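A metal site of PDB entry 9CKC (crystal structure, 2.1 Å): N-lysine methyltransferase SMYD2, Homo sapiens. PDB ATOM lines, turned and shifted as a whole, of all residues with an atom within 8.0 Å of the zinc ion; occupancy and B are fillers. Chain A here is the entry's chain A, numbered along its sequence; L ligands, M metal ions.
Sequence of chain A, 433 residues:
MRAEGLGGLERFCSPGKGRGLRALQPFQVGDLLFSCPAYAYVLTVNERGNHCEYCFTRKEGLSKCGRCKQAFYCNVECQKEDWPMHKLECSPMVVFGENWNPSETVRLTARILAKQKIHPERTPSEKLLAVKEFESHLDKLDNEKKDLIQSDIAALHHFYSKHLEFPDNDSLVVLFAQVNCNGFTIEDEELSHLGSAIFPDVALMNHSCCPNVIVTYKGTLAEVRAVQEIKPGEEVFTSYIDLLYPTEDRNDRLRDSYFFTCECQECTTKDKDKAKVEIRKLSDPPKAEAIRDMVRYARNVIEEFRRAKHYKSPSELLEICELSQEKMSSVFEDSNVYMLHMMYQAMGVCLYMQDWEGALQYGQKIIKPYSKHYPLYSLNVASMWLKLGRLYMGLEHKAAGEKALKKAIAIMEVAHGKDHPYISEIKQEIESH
N of His 207 is in hydrogen-bond range of N3 of the ligand, 3.0 Å away. N4 of the ligand is in hydrogen-bond range of O of His 207 (3.0 Å).
The side-chain sulfur (SG) of Cys 267 lies close to the guanidinium group (NH2) of Arg 250 (3.4 Å). SG of Cys 267 lies close to ND2 of Asn 251 (3.6 Å). A ring nitrogen (NE2) of His 207 lies close to the side-chain sulfur (SG) of Cys 209 (3.2 Å). The side-chain sulfur (SG) of Cys 209 lies close to the guanidinium group (NE) of Arg 250. The side-chain amide oxygen (OD1) of Asn 251 lies within hydrogen-bond range of the backbone NH (N) of Cys 262 (2.9 Å). The side-chain sulfur (SG) of Cys 264 sits close to the backbone NH (N) of Glu 266 (3.5 Å). O of Cys 264 is in hydrogen-bond range of OG1 of Thr 268 (2.8 Å).
Of the 19 residues printed, 4 come within 4 Å of the zinc ion. The nearest printed residue that does not touch the zinc ion is His 207 (4.4 Å).
SG of Cys 267 binds the zinc ion (2.3 Å). The zinc ion is bound by the side-chain sulfur (SG) of Cys 209, at 2.3 Å. The zinc ion is bound by SG of Cys 262. The zinc ion is bound by SG of Cys 264, at 2.4 Å.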
ATOM      1  N   HIS A 207     -26.470  -2.540   6.768  1.00  0.00           N
ATOM      2  CA  HIS A 207     -26.252  -1.892   5.481  1.00  0.00           C
ATOM      3  C   HIS A 207     -27.536  -1.793   4.672  1.00  0.00           C
ATOM      4  O   HIS A 207     -28.377  -2.685   4.685  1.00  0.00           O
ATOM      5  CB  HIS A 207     -25.192  -2.648   4.655  1.00  0.00           C
ATOM      6  CG  HIS A 207     -25.154  -2.239   3.208  1.00  0.00           C
ATOM      7  ND1 HIS A 207     -24.359  -1.207   2.748  1.00  0.00           N
ATOM      8  CD2 HIS A 207     -25.823  -2.702   2.126  1.00  0.00           C
ATOM      9  CE1 HIS A 207     -24.531  -1.067   1.445  1.00  0.00           C
ATOM     10  NE2 HIS A 207     -25.423  -1.965   1.050  1.00  0.00           N
ATOM     11  N   SER A 208     -27.646  -0.694   3.920  1.00  0.00           N
ATOM     12  CA  SER A 208     -28.619  -0.541   2.850  1.00  0.00           C
ATOM     13  C   SER A 208     -27.966   0.242   1.728  1.00  0.00           C
ATOM     14  O   SER A 208     -27.122   1.105   1.971  1.00  0.00           O
ATOM     15  CB  SER A 208     -29.892   0.175   3.317  1.00  0.00           C
ATOM     16  OG  SER A 208     -30.785   0.409   2.237  1.00  0.00           O
ATOM     17  N   CYS A 209     -28.326  -0.087   0.480  1.00  0.00           N
ATOM     18  CA  CYS A 209     -27.867   0.722  -0.651  1.00  0.00           C
ATOM     19  C   CYS A 209     -28.718   1.981  -0.861  1.00  0.00           C
ATOM     20  O   CYS A 209     -28.343   2.833  -1.672  1.00  0.00           O
ATOM     21  CB  CYS A 209     -27.835  -0.111  -1.936  1.00  0.00           C
ATOM     22  SG  CYS A 209     -26.981  -1.729  -1.763  1.00  0.00           S
ATOM     23  N   CYS A 210     -29.816   2.129  -0.126  1.00  0.00           N
ATOM     24  CA  CYS A 210     -30.536   3.400  -0.013  1.00  0.00           C
ATOM     25  C   CYS A 210     -30.595   3.750   1.475  1.00  0.00           C
ATOM     26  O   CYS A 210     -31.663   3.673   2.106  1.00  0.00           O
ATOM     27  CB  CYS A 210     -31.926   3.354  -0.645  1.00  0.00           C
ATOM     28  SG  CYS A 210     -32.806   1.795  -0.487  1.00  0.00           S
ATOM     29  N   ILE A 241     -20.434   0.677   1.358  1.00  0.00           N
ATOM     30  CA  ILE A 241     -19.693   0.615   0.109  1.00  0.00           C
ATOM     31  C   ILE A 241     -19.996   1.836  -0.740  1.00  0.00           C
ATOM     32  O   ILE A 241     -20.921   2.604  -0.467  1.00  0.00           O
ATOM     33  CB  ILE A 241     -20.038  -0.673  -0.683  1.00  0.00           C
ATOM     34  CG1 ILE A 241     -21.545  -0.736  -0.931  1.00  0.00           C
ATOM     35  CG2 ILE A 241     -19.552  -1.909   0.071  1.00  0.00           C
ATOM     36  CD1 ILE A 241     -21.969  -1.765  -1.962  1.00  0.00           C
ATOM     37  N   LEU A 243     -21.701   3.510  -3.639  1.00  0.00           N
ATOM     38  CA  LEU A 243     -23.009   3.210  -4.223  1.00  0.00           C
ATOM     39  C   LEU A 243     -23.093   3.529  -5.721  1.00  0.00           C
ATOM     40  O   LEU A 243     -24.181   3.454  -6.295  1.00  0.00           O
ATOM     41  CB  LEU A 243     -24.107   3.948  -3.456  1.00  0.00           C
ATOM     42  CG  LEU A 243     -24.234   3.511  -1.993  1.00  0.00           C
ATOM     43  CD1 LEU A 243     -25.240   4.365  -1.243  1.00  0.00           C
ATOM     44  CD2 LEU A 243     -24.623   2.032  -1.916  1.00  0.00           C
ATOM     45  N   THR A 247     -26.082  -3.287  -9.333  1.00  0.00           N
ATOM     46  CA  THR A 247     -26.452  -4.173  -8.242  1.00  0.00           C
ATOM     47  C   THR A 247     -25.519  -5.375  -8.137  1.00  0.00           C
ATOM     48  O   THR A 247     -25.161  -5.786  -7.033  1.00  0.00           O
ATOM     49  CB  THR A 247     -27.908  -4.603  -8.416  1.00  0.00           C
ATOM     50  OG1 THR A 247     -28.751  -3.444  -8.390  1.00  0.00           O
ATOM     51  CG2 THR A 247     -28.326  -5.540  -7.284  1.00  0.00           C
ATOM     52  N   ARG A 250     -22.270  -4.212  -6.486  1.00  0.00           N
ATOM     53  CA  ARG A 250     -22.454  -3.955  -5.056  1.00  0.00           C
ATOM     54  C   ARG A 250     -22.565  -5.259  -4.286  1.00  0.00           C
ATOM     55  O   ARG A 250     -21.920  -5.439  -3.239  1.00  0.00           O
ATOM     56  CB  ARG A 250     -23.724  -3.118  -4.840  1.00  0.00           C
ATOM     57  CG  ARG A 250     -23.693  -1.726  -5.461  1.00  0.00           C
ATOM     58  CD  ARG A 250     -24.723  -0.812  -4.820  1.00  0.00           C
ATOM     59  NE  ARG A 250     -26.078  -1.383  -4.838  1.00  0.00           N
ATOM     60  CZ  ARG A 250     -26.876  -1.360  -5.894  1.00  0.00           C
ATOM     61  NH1 ARG A 250     -26.479  -0.805  -7.032  1.00  0.00           N
ATOM     62  NH2 ARG A 250     -28.091  -1.891  -5.826  1.00  0.00           N
ATOM     63  N   ASN A 251     -23.384  -6.171  -4.788  1.00  0.00           N
ATOM     64  CA  ASN A 251     -23.574  -7.415  -4.056  1.00  0.00           C
ATOM     65  C   ASN A 251     -22.365  -8.338  -4.140  1.00  0.00           C
ATOM     66  O   ASN A 251     -22.154  -9.122  -3.213  1.00  0.00           O
ATOM     67  CB  ASN A 251     -24.849  -8.123  -4.530  1.00  0.00           C
ATOM     68  CG  ASN A 251     -26.041  -7.766  -3.666  1.00  0.00           C
ATOM     69  OD1 ASN A 251     -25.967  -7.810  -2.443  1.00  0.00           O
ATOM     70  ND2 ASN A 251     -27.157  -7.395  -4.300  1.00  0.00           N
ATOM     71  N   LEU A 254     -20.349  -6.824  -1.221  1.00  0.00           N
ATOM     72  CA  LEU A 254     -20.966  -7.110   0.074  1.00  0.00           C
ATOM     73  C   LEU A 254     -20.827  -8.568   0.464  1.00  0.00           C
ATOM     74  O   LEU A 254     -20.541  -8.892   1.620  1.00  0.00           O
ATOM     75  CB  LEU A 254     -22.438  -6.695   0.053  1.00  0.00           C
ATOM     76  CG  LEU A 254     -22.731  -5.213  -0.117  1.00  0.00           C
ATOM     77  CD1 LEU A 254     -24.229  -4.989  -0.245  1.00  0.00           C
ATOM     78  CD2 LEU A 254     -22.147  -4.412   1.034  1.00  0.00           C
ATOM     79  N   PHE A 260     -23.071 -11.354   3.145  1.00  0.00           N
ATOM     80  CA  PHE A 260     -24.511 -11.278   3.042  1.00  0.00           C
ATOM     81  C   PHE A 260     -24.868 -10.742   1.664  1.00  0.00           C
ATOM     82  O   PHE A 260     -24.070 -10.079   1.008  1.00  0.00           O
ATOM     83  CB  PHE A 260     -25.124 -10.398   4.137  1.00  0.00           C
ATOM     84  CG  PHE A 260     -24.953  -8.918   3.908  1.00  0.00           C
ATOM     85  CD1 PHE A 260     -23.819  -8.257   4.358  1.00  0.00           C
ATOM     86  CD2 PHE A 260     -25.940  -8.175   3.262  1.00  0.00           C
ATOM     87  CE1 PHE A 260     -23.657  -6.895   4.148  1.00  0.00           C
ATOM     88  CE2 PHE A 260     -25.787  -6.815   3.057  1.00  0.00           C
ATOM     89  CZ  PHE A 260     -24.638  -6.171   3.506  1.00  0.00           C
ATOM     90  N   THR A 261     -26.103 -11.036   1.244  1.00  0.00           N
ATOM     91  CA  THR A 261     -26.678 -10.531   0.007  1.00  0.00           C
ATOM     92  C   THR A 261     -27.733  -9.502   0.366  1.00  0.00           C
ATOM     93  O   THR A 261     -28.715  -9.829   1.053  1.00  0.00           O
ATOM     94  CB  THR A 261     -27.304 -11.671  -0.796  1.00  0.00           C
ATOM     95  OG1 THR A 261     -26.308 -12.650  -1.092  1.00  0.00           O
ATOM     96  CG2 THR A 261     -27.902 -11.133  -2.084  1.00  0.00           C
ATOM     97  N   CYS A 262     -27.555  -8.271  -0.110  1.00  0.00           N
ATOM     98  CA  CYS A 262     -28.453  -7.188   0.240  1.00  0.00           C
ATOM     99  C   CYS A 262     -29.805  -7.346  -0.455  1.00  0.00           C
ATOM    100  O   CYS A 262     -29.875  -7.776  -1.609  1.00  0.00           O
ATOM    101  CB  CYS A 262     -27.812  -5.852  -0.141  1.00  0.00           C
ATOM    102  SG  CYS A 262     -28.724  -4.422   0.419  1.00  0.00           S
ATOM    103  N   GLU A 263     -30.874  -6.975   0.256  1.00  0.00           N
ATOM    104  CA  GLU A 263     -32.230  -7.054  -0.260  1.00  0.00           C
ATOM    105  C   GLU A 263     -32.955  -5.714  -0.128  1.00  0.00           C
ATOM    106  O   GLU A 263     -34.191  -5.677  -0.079  1.00  0.00           O
ATOM    107  CB  GLU A 263     -33.024  -8.154   0.437  1.00  0.00           C
ATOM    108  CG  GLU A 263     -32.476  -9.551   0.206  1.00  0.00           C
ATOM    109  CD  GLU A 263     -33.236 -10.618   0.980  1.00  0.00           C
ATOM    110  OE1 GLU A 263     -34.272 -10.291   1.602  1.00  0.00           O
ATOM    111  OE2 GLU A 263     -32.781 -11.779   0.981  1.00  0.00           O
ATOM    112  N   CYS A 264     -32.210  -4.616  -0.103  1.00  0.00           N
ATOM    113  CA  CYS A 264     -32.842  -3.302  -0.069  1.00  0.00           C
ATOM    114  C   CYS A 264     -33.596  -3.045  -1.381  1.00  0.00           C
ATOM    115  O   CYS A 264     -33.531  -3.841  -2.323  1.00  0.00           O
ATOM    116  CB  CYS A 264     -31.789  -2.212   0.165  1.00  0.00           C
ATOM    117  SG  CYS A 264     -30.813  -1.776  -1.301  1.00  0.00           S
ATOM    118  N   GLN A 265     -34.341  -1.941  -1.409  1.00  0.00           N
ATOM    119  CA  GLN A 265     -35.169  -1.628  -2.573  1.00  0.00           C
ATOM    120  C   GLN A 265     -34.321  -1.481  -3.838  1.00  0.00           C
ATOM    121  O   GLN A 265     -34.736  -1.938  -4.915  1.00  0.00           O
ATOM    122  CB  GLN A 265     -35.972  -0.353  -2.332  1.00  0.00           C
ATOM    123  CG  GLN A 265     -37.044  -0.121  -3.382  1.00  0.00           C
ATOM    124  CD  GLN A 265     -37.919   1.082  -3.068  1.00  0.00           C
ATOM    125  OE1 GLN A 265     -37.429   2.113  -2.615  1.00  0.00           O
ATOM    126  NE2 GLN A 265     -39.217   0.951  -3.319  1.00  0.00           N
ATOM    127  N   GLU A 266     -33.156  -0.828  -3.750  1.00  0.00           N
ATOM    128  CA  GLU A 266     -32.295  -0.673  -4.919  1.00  0.00           C
ATOM    129  C   GLU A 266     -31.844  -2.031  -5.451  1.00  0.00           C
ATOM    130  O   GLU A 266     -31.837  -2.243  -6.672  1.00  0.00           O
ATOM    131  CB  GLU A 266     -31.091   0.198  -4.599  1.00  0.00           C
ATOM    132  CG  GLU A 266     -31.404   1.673  -4.479  1.00  0.00           C
ATOM    133  CD  GLU A 266     -31.863   2.274  -5.805  1.00  0.00           C
ATOM    134  OE1 GLU A 266     -31.565   1.682  -6.874  1.00  0.00           O
ATOM    135  OE2 GLU A 266     -32.536   3.329  -5.784  1.00  0.00           O
ATOM    136  N   CYS A 267     -31.454  -2.950  -4.569  1.00  0.00           N
ATOM    137  CA  CYS A 267     -31.024  -4.271  -5.014  1.00  0.00           C
ATOM    138  C   CYS A 267     -32.201  -5.096  -5.528  1.00  0.00           C
ATOM    139  O   CYS A 267     -32.057  -5.848  -6.498  1.00  0.00           O
ATOM    140  CB  CYS A 267     -30.300  -5.001  -3.876  1.00  0.00           C
ATOM    141  SG  CYS A 267     -28.698  -4.283  -3.476  1.00  0.00           S
ATOM    142  N   THR A 268     -33.366  -4.964  -4.885  1.00  0.00           N
ATOM    143  CA  THR A 268     -34.541  -5.735  -5.282  1.00  0.00           C
ATOM    144  C   THR A 268     -35.065  -5.300  -6.650  1.00  0.00           C
ATOM    145  O   THR A 268     -35.342  -6.133  -7.512  1.00  0.00           O
ATOM    146  CB  THR A 268     -35.628  -5.595  -4.221  1.00  0.00           C
ATOM    147  OG1 THR A 268     -35.151  -6.089  -2.970  1.00  0.00           O
ATOM    148  CG2 THR A 268     -36.880  -6.372  -4.617  1.00  0.00           C
HETATM  149  N1  LIG L   1     -25.759  -7.217  12.136  1.00  0.00           N
HETATM  150  C1  LIG L   1     -24.423  -7.021  12.706  1.00  0.00           C
HETATM  151  C2  LIG L   1     -24.089  -5.535  12.813  1.00  0.00           C
HETATM  152  C3  LIG L   1     -23.439  -4.954  11.555  1.00  0.00           C
HETATM  153  S1  LIG L   1     -21.746  -5.553  11.325  1.00  0.00           S
HETATM  154  C4  LIG L   1     -24.300  -7.716  14.053  1.00  0.00           C
HETATM  155  O1  LIG L   1     -25.196  -8.451  14.489  1.00  0.00           O
HETATM  156  O2  LIG L   1     -23.285  -7.586  14.729  1.00  0.00           O
HETATM  157  C5  LIG L   1     -21.963  -6.167   9.635  1.00  0.00           C
HETATM  158  C6  LIG L   1     -22.700  -7.497   9.507  1.00  0.00           C
HETATM  159  O3  LIG L   1     -24.101  -7.324   9.674  1.00  0.00           O
HETATM  160  C7  LIG L   1     -22.530  -8.098   8.123  1.00  0.00           C
HETATM  161  O4  LIG L   1     -21.365  -8.883   8.035  1.00  0.00           O
HETATM  162  C8  LIG L   1     -23.781  -8.930   7.971  1.00  0.00           C
HETATM  163  O5  LIG L   1     -23.587 -10.135   8.663  1.00  0.00           O
HETATM  164  C9  LIG L   1     -24.805  -8.130   8.751  1.00  0.00           C
HETATM  165  N2  LIG L   1     -25.579  -7.271   7.836  1.00  0.00           N
HETATM  166  C10 LIG L   1     -25.394  -5.924   7.622  1.00  0.00           C
HETATM  167  N3  LIG L   1     -26.305  -5.507   6.718  1.00  0.00           N
HETATM  168  C11 LIG L   1     -27.078  -6.563   6.351  1.00  0.00           C
HETATM  169  C12 LIG L   1     -28.143  -6.713   5.459  1.00  0.00           C
HETATM  170  N4  LIG L   1     -28.615  -5.684   4.775  1.00  0.00           N
HETATM  171  N5  LIG L   1     -28.722  -7.952   5.295  1.00  0.00           N
HETATM  172  C13 LIG L   1     -28.260  -9.033   6.005  1.00  0.00           C
HETATM  173  N6  LIG L   1     -27.205  -8.881   6.877  1.00  0.00           N
HETATM  174  C14 LIG L   1     -26.624  -7.671   7.053  1.00  0.00           C
HETATM  175 ZN    ZN M   1     -28.830  -3.096  -1.504  1.00  0.00          ZN
